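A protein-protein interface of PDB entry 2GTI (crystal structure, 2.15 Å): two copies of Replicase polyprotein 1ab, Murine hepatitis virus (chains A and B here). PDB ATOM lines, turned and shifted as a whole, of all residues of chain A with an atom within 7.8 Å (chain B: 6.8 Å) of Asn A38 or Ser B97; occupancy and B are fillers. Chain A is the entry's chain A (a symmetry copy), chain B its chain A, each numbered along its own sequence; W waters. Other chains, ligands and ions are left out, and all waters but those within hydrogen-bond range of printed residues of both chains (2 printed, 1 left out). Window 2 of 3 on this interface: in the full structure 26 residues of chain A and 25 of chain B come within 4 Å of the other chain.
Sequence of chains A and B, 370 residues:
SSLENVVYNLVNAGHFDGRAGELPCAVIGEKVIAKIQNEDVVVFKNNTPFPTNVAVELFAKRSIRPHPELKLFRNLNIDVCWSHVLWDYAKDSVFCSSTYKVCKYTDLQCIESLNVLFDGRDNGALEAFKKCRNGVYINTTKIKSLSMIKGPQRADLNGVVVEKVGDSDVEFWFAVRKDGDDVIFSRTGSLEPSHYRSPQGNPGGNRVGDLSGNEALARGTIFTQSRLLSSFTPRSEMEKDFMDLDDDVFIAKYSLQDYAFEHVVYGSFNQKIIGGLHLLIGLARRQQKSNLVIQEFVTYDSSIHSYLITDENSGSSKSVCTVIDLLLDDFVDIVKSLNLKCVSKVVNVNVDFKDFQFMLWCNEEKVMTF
NZ of Lys B91 is in salt-bridge range of OE2 of Glu A39 (2.7 Å).
NZ of Lys B91 is in hydrogen-bond range of O of Asp A40, at 3.1 Å.
The side-chain carboxylate of Glu A39 sits close to the backbone carbonyl oxygen of Phe B95, at 3.4 Å.
No position is printed for both chains.
O of Asn A38 touches OG of Ser B97, 3.8 Å away.
Asp A40 touches Ser B97 (OD2 to CB, 3.3 Å).
Asn A38 touches one residue of chain B.
Of the printed residues of chain B, Glu A39 touches Lys B91 (2.7 Å) and Phe B95 (3.4 Å).
Of the printed residues of chain B, Asp A40 touches Lys B91 (3.1 Å) and Ser B97 (3.3 Å).
Val A41 touches none of the printed residues of chain B.
Of the printed residues of chain A, Lys B91 touches Glu A39 and Asp A40.
Printed residues of chain A within 4 Å of Phe B95: Glu A39.
Thr B99 touches none of the printed residues of chain A.
The nearest residue of chain A that does not touch Ser B97 is Glu A39 (4.8 Å).
The nearest printed residue of chain B that does not touch Glu A39 is Ser B97 (4.8 Å).
Water W2 lies within hydrogen-bond range of the backbone NH of Ser B97 (2.8 Å) and the backbone carbonyl oxygen of Asn A38 (3.0 Å).
Water W1 lies within hydrogen-bond range of O of Asp A40 (2.9 Å), NZ of Lys B91 (3.3 Å) and O of Val B94 (3.4 Å).
O of Val B94 lies within hydrogen-bond range of NZ of Lys B91 (2.9 Å).
The side-chain amino group (NZ) of Lys B91 lies within hydrogen-bond range of the backbone carbonyl oxygen (O) of Phe B95 (3.2 Å).
The side-chain amino group of Lys A35 is in salt-bridge range of the side-chain carboxylate of Asp A40 (2.7 Å).
Of the 8 printed residues of chain A, 3 touch a printed residue of chain B.
Printed residues of chain A that touch a printed residue of chain B: Asn A38, Glu A39 and Asp A40.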
ATOM      1  N   ALA A  34       3.610 -26.265   4.291  1.00  0.00           N
ATOM      2  CA  ALA A  34       2.921 -27.202   3.412  1.00  0.00           C
ATOM      3  C   ALA A  34       1.525 -27.429   3.946  1.00  0.00           C
ATOM      4  O   ALA A  34       1.321 -27.453   5.158  1.00  0.00           O
ATOM      5  CB  ALA A  34       3.657 -28.529   3.353  1.00  0.00           C
ATOM      6  N   LYS A  35       0.564 -27.579   3.044  1.00  0.00           N
ATOM      7  CA  LYS A  35      -0.806 -27.841   3.447  1.00  0.00           C
ATOM      8  C   LYS A  35      -0.958 -29.355   3.399  1.00  0.00           C
ATOM      9  O   LYS A  35      -0.979 -29.956   2.326  1.00  0.00           O
ATOM     10  CB  LYS A  35      -1.799 -27.170   2.495  1.00  0.00           C
ATOM     11  CG  LYS A  35      -3.225 -27.136   3.037  1.00  0.00           C
ATOM     12  CD  LYS A  35      -4.161 -26.283   2.175  1.00  0.00           C
ATOM     13  CE  LYS A  35      -3.733 -24.811   2.140  1.00  0.00           C
ATOM     14  NZ  LYS A  35      -3.832 -24.107   3.458  1.00  0.00           N
ATOM     15  N   ILE A  36      -1.030 -29.968   4.572  1.00  0.00           N
ATOM     16  CA  ILE A  36      -1.163 -31.412   4.676  1.00  0.00           C
ATOM     17  C   ILE A  36      -2.461 -31.758   5.392  1.00  0.00           C
ATOM     18  O   ILE A  36      -2.657 -31.384   6.545  1.00  0.00           O
ATOM     19  CB  ILE A  36       0.023 -32.014   5.455  1.00  0.00           C
ATOM     20  CG1 ILE A  36       1.334 -31.675   4.738  1.00  0.00           C
ATOM     21  CG2 ILE A  36      -0.142 -33.529   5.567  1.00  0.00           C
ATOM     22  CD1 ILE A  36       2.571 -32.047   5.524  1.00  0.00           C
ATOM     23  N   GLN A  37      -3.344 -32.475   4.699  1.00  0.00           N
ATOM     24  CA  GLN A  37      -4.634 -32.854   5.258  1.00  0.00           C
ATOM     25  C   GLN A  37      -5.371 -31.595   5.695  1.00  0.00           C
ATOM     26  O   GLN A  37      -5.901 -31.524   6.806  1.00  0.00           O
ATOM     27  CB  GLN A  37      -4.455 -33.785   6.459  1.00  0.00           C
ATOM     28  CG  GLN A  37      -5.105 -35.149   6.293  1.00  0.00           C
ATOM     29  CD  GLN A  37      -4.296 -36.079   5.414  1.00  0.00           C
ATOM     30  OE1 GLN A  37      -4.794 -37.111   4.962  1.00  0.00           O
ATOM     31  NE2 GLN A  37      -3.038 -35.726   5.176  1.00  0.00           N
ATOM     32  N   ASN A  38      -5.383 -30.601   4.811  1.00  0.00           N
ATOM     33  CA  ASN A  38      -6.050 -29.329   5.060  1.00  0.00           C
ATOM     34  C   ASN A  38      -5.490 -28.562   6.259  1.00  0.00           C
ATOM     35  O   ASN A  38      -6.111 -27.616   6.747  1.00  0.00           O
ATOM     36  CB  ASN A  38      -7.546 -29.558   5.265  1.00  0.00           C
ATOM     37  CG  ASN A  38      -8.390 -28.587   4.475  1.00  0.00           C
ATOM     38  OD1 ASN A  38      -8.427 -28.635   3.246  1.00  0.00           O
ATOM     39  ND2 ASN A  38      -9.067 -27.691   5.176  1.00  0.00           N
ATOM     40  N   GLU A  39      -4.315 -28.970   6.727  1.00  0.00           N
ATOM     41  CA  GLU A  39      -3.662 -28.321   7.861  1.00  0.00           C
ATOM     42  C   GLU A  39      -2.353 -27.704   7.368  1.00  0.00           C
ATOM     43  O   GLU A  39      -1.700 -28.258   6.488  1.00  0.00           O
ATOM     44  CB  GLU A  39      -3.367 -29.361   8.954  1.00  0.00           C
ATOM     45  CG  GLU A  39      -2.822 -28.784  10.249  1.00  0.00           C
ATOM     46  CD  GLU A  39      -2.506 -29.852  11.285  1.00  0.00           C
ATOM     47  OE1 GLU A  39      -2.995 -30.993  11.149  1.00  0.00           O
ATOM     48  OE2 GLU A  39      -1.779 -29.546  12.251  1.00  0.00           O
ATOM     49  N   ASP A  40      -1.969 -26.563   7.932  1.00  0.00           N
ATOM     50  CA  ASP A  40      -0.721 -25.908   7.531  1.00  0.00           C
ATOM     51  C   ASP A  40       0.394 -26.234   8.513  1.00  0.00           C
ATOM     52  O   ASP A  40       0.270 -25.991   9.711  1.00  0.00           O
ATOM     53  CB  ASP A  40      -0.901 -24.388   7.443  1.00  0.00           C
ATOM     54  CG  ASP A  40      -1.927 -23.985   6.403  1.00  0.00           C
ATOM     55  OD1 ASP A  40      -2.011 -24.661   5.361  1.00  0.00           O
ATOM     56  OD2 ASP A  40      -2.641 -22.986   6.616  1.00  0.00           O
ATOM     57  N   VAL A  41       1.490 -26.781   7.998  1.00  0.00           N
ATOM     58  CA  VAL A  41       2.616 -27.152   8.845  1.00  0.00           C
ATOM     59  C   VAL A  41       3.961 -26.697   8.288  1.00  0.00           C
ATOM     60  O   VAL A  41       4.222 -26.810   7.087  1.00  0.00           O
ATOM     61  CB  VAL A  41       2.653 -28.687   9.056  1.00  0.00           C
ATOM     62  CG1 VAL A  41       2.600 -29.387   7.723  1.00  0.00           C
ATOM     63  CG2 VAL A  41       3.915 -29.090   9.807  1.00  0.00           C
ATOM     64  N   PRO B  49       1.952 -19.775  10.176  1.00  0.00           N
ATOM     65  CA  PRO B  49       1.771 -19.263   8.815  1.00  0.00           C
ATOM     66  C   PRO B  49       1.004 -17.943   8.813  1.00  0.00           C
ATOM     67  O   PRO B  49       0.760 -17.360   7.760  1.00  0.00           O
ATOM     68  CB  PRO B  49       0.991 -20.382   8.136  1.00  0.00           C
ATOM     69  CG  PRO B  49       0.116 -20.866   9.247  1.00  0.00           C
ATOM     70  CD  PRO B  49       1.060 -20.923  10.427  1.00  0.00           C
ATOM     71  N   PHE B  50       0.639 -17.476  10.004  1.00  0.00           N
ATOM     72  CA  PHE B  50      -0.123 -16.235  10.169  1.00  0.00           C
ATOM     73  C   PHE B  50       0.741 -14.987  10.335  1.00  0.00           C
ATOM     74  O   PHE B  50       1.925 -15.075  10.668  1.00  0.00           O
ATOM     75  CB  PHE B  50      -1.016 -16.321  11.412  1.00  0.00           C
ATOM     76  CG  PHE B  50      -2.015 -17.441  11.384  1.00  0.00           C
ATOM     77  CD1 PHE B  50      -3.135 -17.376  10.559  1.00  0.00           C
ATOM     78  CD2 PHE B  50      -1.857 -18.550  12.217  1.00  0.00           C
ATOM     79  CE1 PHE B  50      -4.087 -18.397  10.567  1.00  0.00           C
ATOM     80  CE2 PHE B  50      -2.803 -19.574  12.232  1.00  0.00           C
ATOM     81  CZ  PHE B  50      -3.920 -19.499  11.407  1.00  0.00           C
ATOM     82  N   ILE B  78     -10.834 -33.127  11.988  1.00  0.00           N
ATOM     83  CA  ILE B  78     -11.387 -31.852  12.443  1.00  0.00           C
ATOM     84  C   ILE B  78     -10.841 -30.735  11.552  1.00  0.00           C
ATOM     85  O   ILE B  78      -9.640 -30.673  11.309  1.00  0.00           O
ATOM     86  CB  ILE B  78     -10.993 -31.553  13.928  1.00  0.00           C
ATOM     87  CG1 ILE B  78     -11.943 -32.271  14.891  1.00  0.00           C
ATOM     88  CG2 ILE B  78     -11.106 -30.057  14.214  1.00  0.00           C
ATOM     89  CD1 ILE B  78     -12.192 -33.696  14.578  1.00  0.00           C
ATOM     90  N   ASP B  79     -11.722 -29.856  11.080  1.00  0.00           N
ATOM     91  CA  ASP B  79     -11.322 -28.743  10.219  1.00  0.00           C
ATOM     92  C   ASP B  79     -11.194 -27.425  10.977  1.00  0.00           C
ATOM     93  O   ASP B  79     -10.376 -26.586  10.634  1.00  0.00           O
ATOM     94  CB  ASP B  79     -12.334 -28.548   9.084  1.00  0.00           C
ATOM     95  CG  ASP B  79     -12.361 -29.713   8.114  1.00  0.00           C
ATOM     96  OD1 ASP B  79     -11.276 -30.137   7.673  1.00  0.00           O
ATOM     97  OD2 ASP B  79     -13.467 -30.198   7.783  1.00  0.00           O
ATOM     98  N   VAL B  80     -12.012 -27.233  12.002  1.00  0.00           N
ATOM     99  CA  VAL B  80     -11.968 -25.990  12.758  1.00  0.00           C
ATOM    100  C   VAL B  80     -12.571 -26.185  14.133  1.00  0.00           C
ATOM    101  O   VAL B  80     -13.405 -27.066  14.324  1.00  0.00           O
ATOM    102  CB  VAL B  80     -12.738 -24.856  12.017  1.00  0.00           C
ATOM    103  CG1 VAL B  80     -14.215 -25.241  11.831  1.00  0.00           C
ATOM    104  CG2 VAL B  80     -12.616 -23.548  12.795  1.00  0.00           C
ATOM    105  N   LYS B  91       4.141 -28.779  17.155  1.00  0.00           N
ATOM    106  CA  LYS B  91       4.158 -28.079  15.885  1.00  0.00           C
ATOM    107  C   LYS B  91       4.590 -26.627  16.081  1.00  0.00           C
ATOM    108  O   LYS B  91       5.116 -25.995  15.163  1.00  0.00           O
ATOM    109  CB  LYS B  91       2.751 -28.138  15.276  1.00  0.00           C
ATOM    110  CG  LYS B  91       2.672 -27.766  13.819  1.00  0.00           C
ATOM    111  CD  LYS B  91       1.284 -28.050  13.240  1.00  0.00           C
ATOM    112  CE  LYS B  91       0.395 -26.820  13.253  1.00  0.00           C
ATOM    113  NZ  LYS B  91      -0.816 -26.998  12.406  1.00  0.00           N
ATOM    114  N   VAL B  94      -0.762 -23.084  15.797  1.00  0.00           N
ATOM    115  CA  VAL B  94      -2.142 -23.439  16.077  1.00  0.00           C
ATOM    116  C   VAL B  94      -2.449 -24.754  15.369  1.00  0.00           C
ATOM    117  O   VAL B  94      -1.800 -25.097  14.374  1.00  0.00           O
ATOM    118  CB  VAL B  94      -3.118 -22.349  15.568  1.00  0.00           C
ATOM    119  CG1 VAL B  94      -4.541 -22.778  15.816  1.00  0.00           C
ATOM    120  CG2 VAL B  94      -2.856 -21.035  16.283  1.00  0.00           C
ATOM    121  N   PHE B  95      -3.428 -25.488  15.885  1.00  0.00           N
ATOM    122  CA  PHE B  95      -3.826 -26.768  15.303  1.00  0.00           C
ATOM    123  C   PHE B  95      -4.492 -26.599  13.935  1.00  0.00           C
ATOM    124  O   PHE B  95      -3.957 -27.041  12.920  1.00  0.00           O
ATOM    125  CB  PHE B  95      -4.765 -27.506  16.263  1.00  0.00           C
ATOM    126  CG  PHE B  95      -5.432 -28.713  15.661  1.00  0.00           C
ATOM    127  CD1 PHE B  95      -4.721 -29.585  14.837  1.00  0.00           C
ATOM    128  CD2 PHE B  95      -6.764 -28.992  15.939  1.00  0.00           C
ATOM    129  CE1 PHE B  95      -5.329 -30.720  14.299  1.00  0.00           C
ATOM    130  CE2 PHE B  95      -7.386 -30.121  15.409  1.00  0.00           C
ATOM    131  CZ  PHE B  95      -6.665 -30.991  14.585  1.00  0.00           C
ATOM    132  N   CYS B  96      -5.658 -25.966  13.909  1.00  0.00           N
ATOM    133  CA  CYS B  96      -6.370 -25.751  12.652  1.00  0.00           C
ATOM    134  C   CYS B  96      -5.838 -24.533  11.901  1.00  0.00           C
ATOM    135  O   CYS B  96      -5.316 -23.592  12.505  1.00  0.00           O
ATOM    136  CB  CYS B  96      -7.864 -25.581  12.918  1.00  0.00           C
ATOM    137  SG  CYS B  96      -8.589 -27.013  13.731  1.00  0.00           S
ATOM    138  N   SER B  97      -5.971 -24.551  10.581  1.00  0.00           N
ATOM    139  CA  SER B  97      -5.490 -23.436   9.786  1.00  0.00           C
ATOM    140  C   SER B  97      -6.472 -22.275   9.839  1.00  0.00           C
ATOM    141  O   SER B  97      -6.157 -21.176   9.396  1.00  0.00           O
ATOM    142  CB  SER B  97      -5.259 -23.865   8.332  1.00  0.00           C
ATOM    143  OG  SER B  97      -6.477 -23.954   7.616  1.00  0.00           O
ATOM    144  N   SER B  98      -7.661 -22.515  10.384  1.00  0.00           N
ATOM    145  CA  SER B  98      -8.667 -21.459  10.493  1.00  0.00           C
ATOM    146  C   SER B  98      -9.360 -21.444  11.848  1.00  0.00           C
ATOM    147  O   SER B  98      -9.297 -22.416  12.603  1.00  0.00           O
ATOM    148  CB  SER B  98      -9.716 -21.604   9.388  1.00  0.00           C
ATOM    149  OG  SER B  98      -9.167 -21.280   8.121  1.00  0.00           O
ATOM    150  N   THR B  99     -10.015 -20.330  12.157  1.00  0.00           N
ATOM    151  CA  THR B  99     -10.721 -20.207  13.425  1.00  0.00           C
ATOM    152  C   THR B  99     -12.183 -19.861  13.208  1.00  0.00           C
ATOM    153  O   THR B  99     -12.608 -19.561  12.094  1.00  0.00           O
ATOM    154  CB  THR B  99     -10.103 -19.108  14.332  1.00  0.00           C
ATOM    155  OG1 THR B  99     -10.204 -17.830  13.686  1.00  0.00           O
ATOM    156  CG2 THR B  99      -8.644 -19.415  14.633  1.00  0.00           C
ATOM    157  N   THR B 106      -8.842 -13.919  11.304  1.00  0.00           N
ATOM    158  CA  THR B 106      -8.775 -15.282  10.790  1.00  0.00           C
ATOM    159  C   THR B 106     -10.080 -16.082  10.802  1.00  0.00           C
ATOM    160  O   THR B 106     -10.150 -17.154  10.198  1.00  0.00           O
ATOM    161  CB  THR B 106      -7.730 -16.090  11.569  1.00  0.00           C
ATOM    162  OG1 THR B 106      -8.094 -16.118  12.951  1.00  0.00           O
ATOM    163  CG2 THR B 106      -6.343 -15.458  11.434  1.00  0.00           C
ATOM    164  N   LEU B 114     -17.844 -27.815   7.113  1.00  0.00           N
ATOM    165  CA  LEU B 114     -16.596 -28.289   7.693  1.00  0.00           C
ATOM    166  C   LEU B 114     -16.858 -29.175   8.913  1.00  0.00           C
ATOM    167  O   LEU B 114     -17.939 -29.140   9.493  1.00  0.00           O
ATOM    168  CB  LEU B 114     -15.708 -27.108   8.099  1.00  0.00           C
ATOM    169  CG  LEU B 114     -15.392 -26.051   7.036  1.00  0.00           C
ATOM    170  CD1 LEU B 114     -14.332 -25.117   7.580  1.00  0.00           C
ATOM    171  CD2 LEU B 114     -14.909 -26.704   5.759  1.00  0.00           C
HETATM  172  O   HOH W   1      -0.127 -23.875  11.715  1.00  0.00           O
HETATM  173  O   HOH W   2      -6.846 -26.993   9.536  1.00  0.00           O
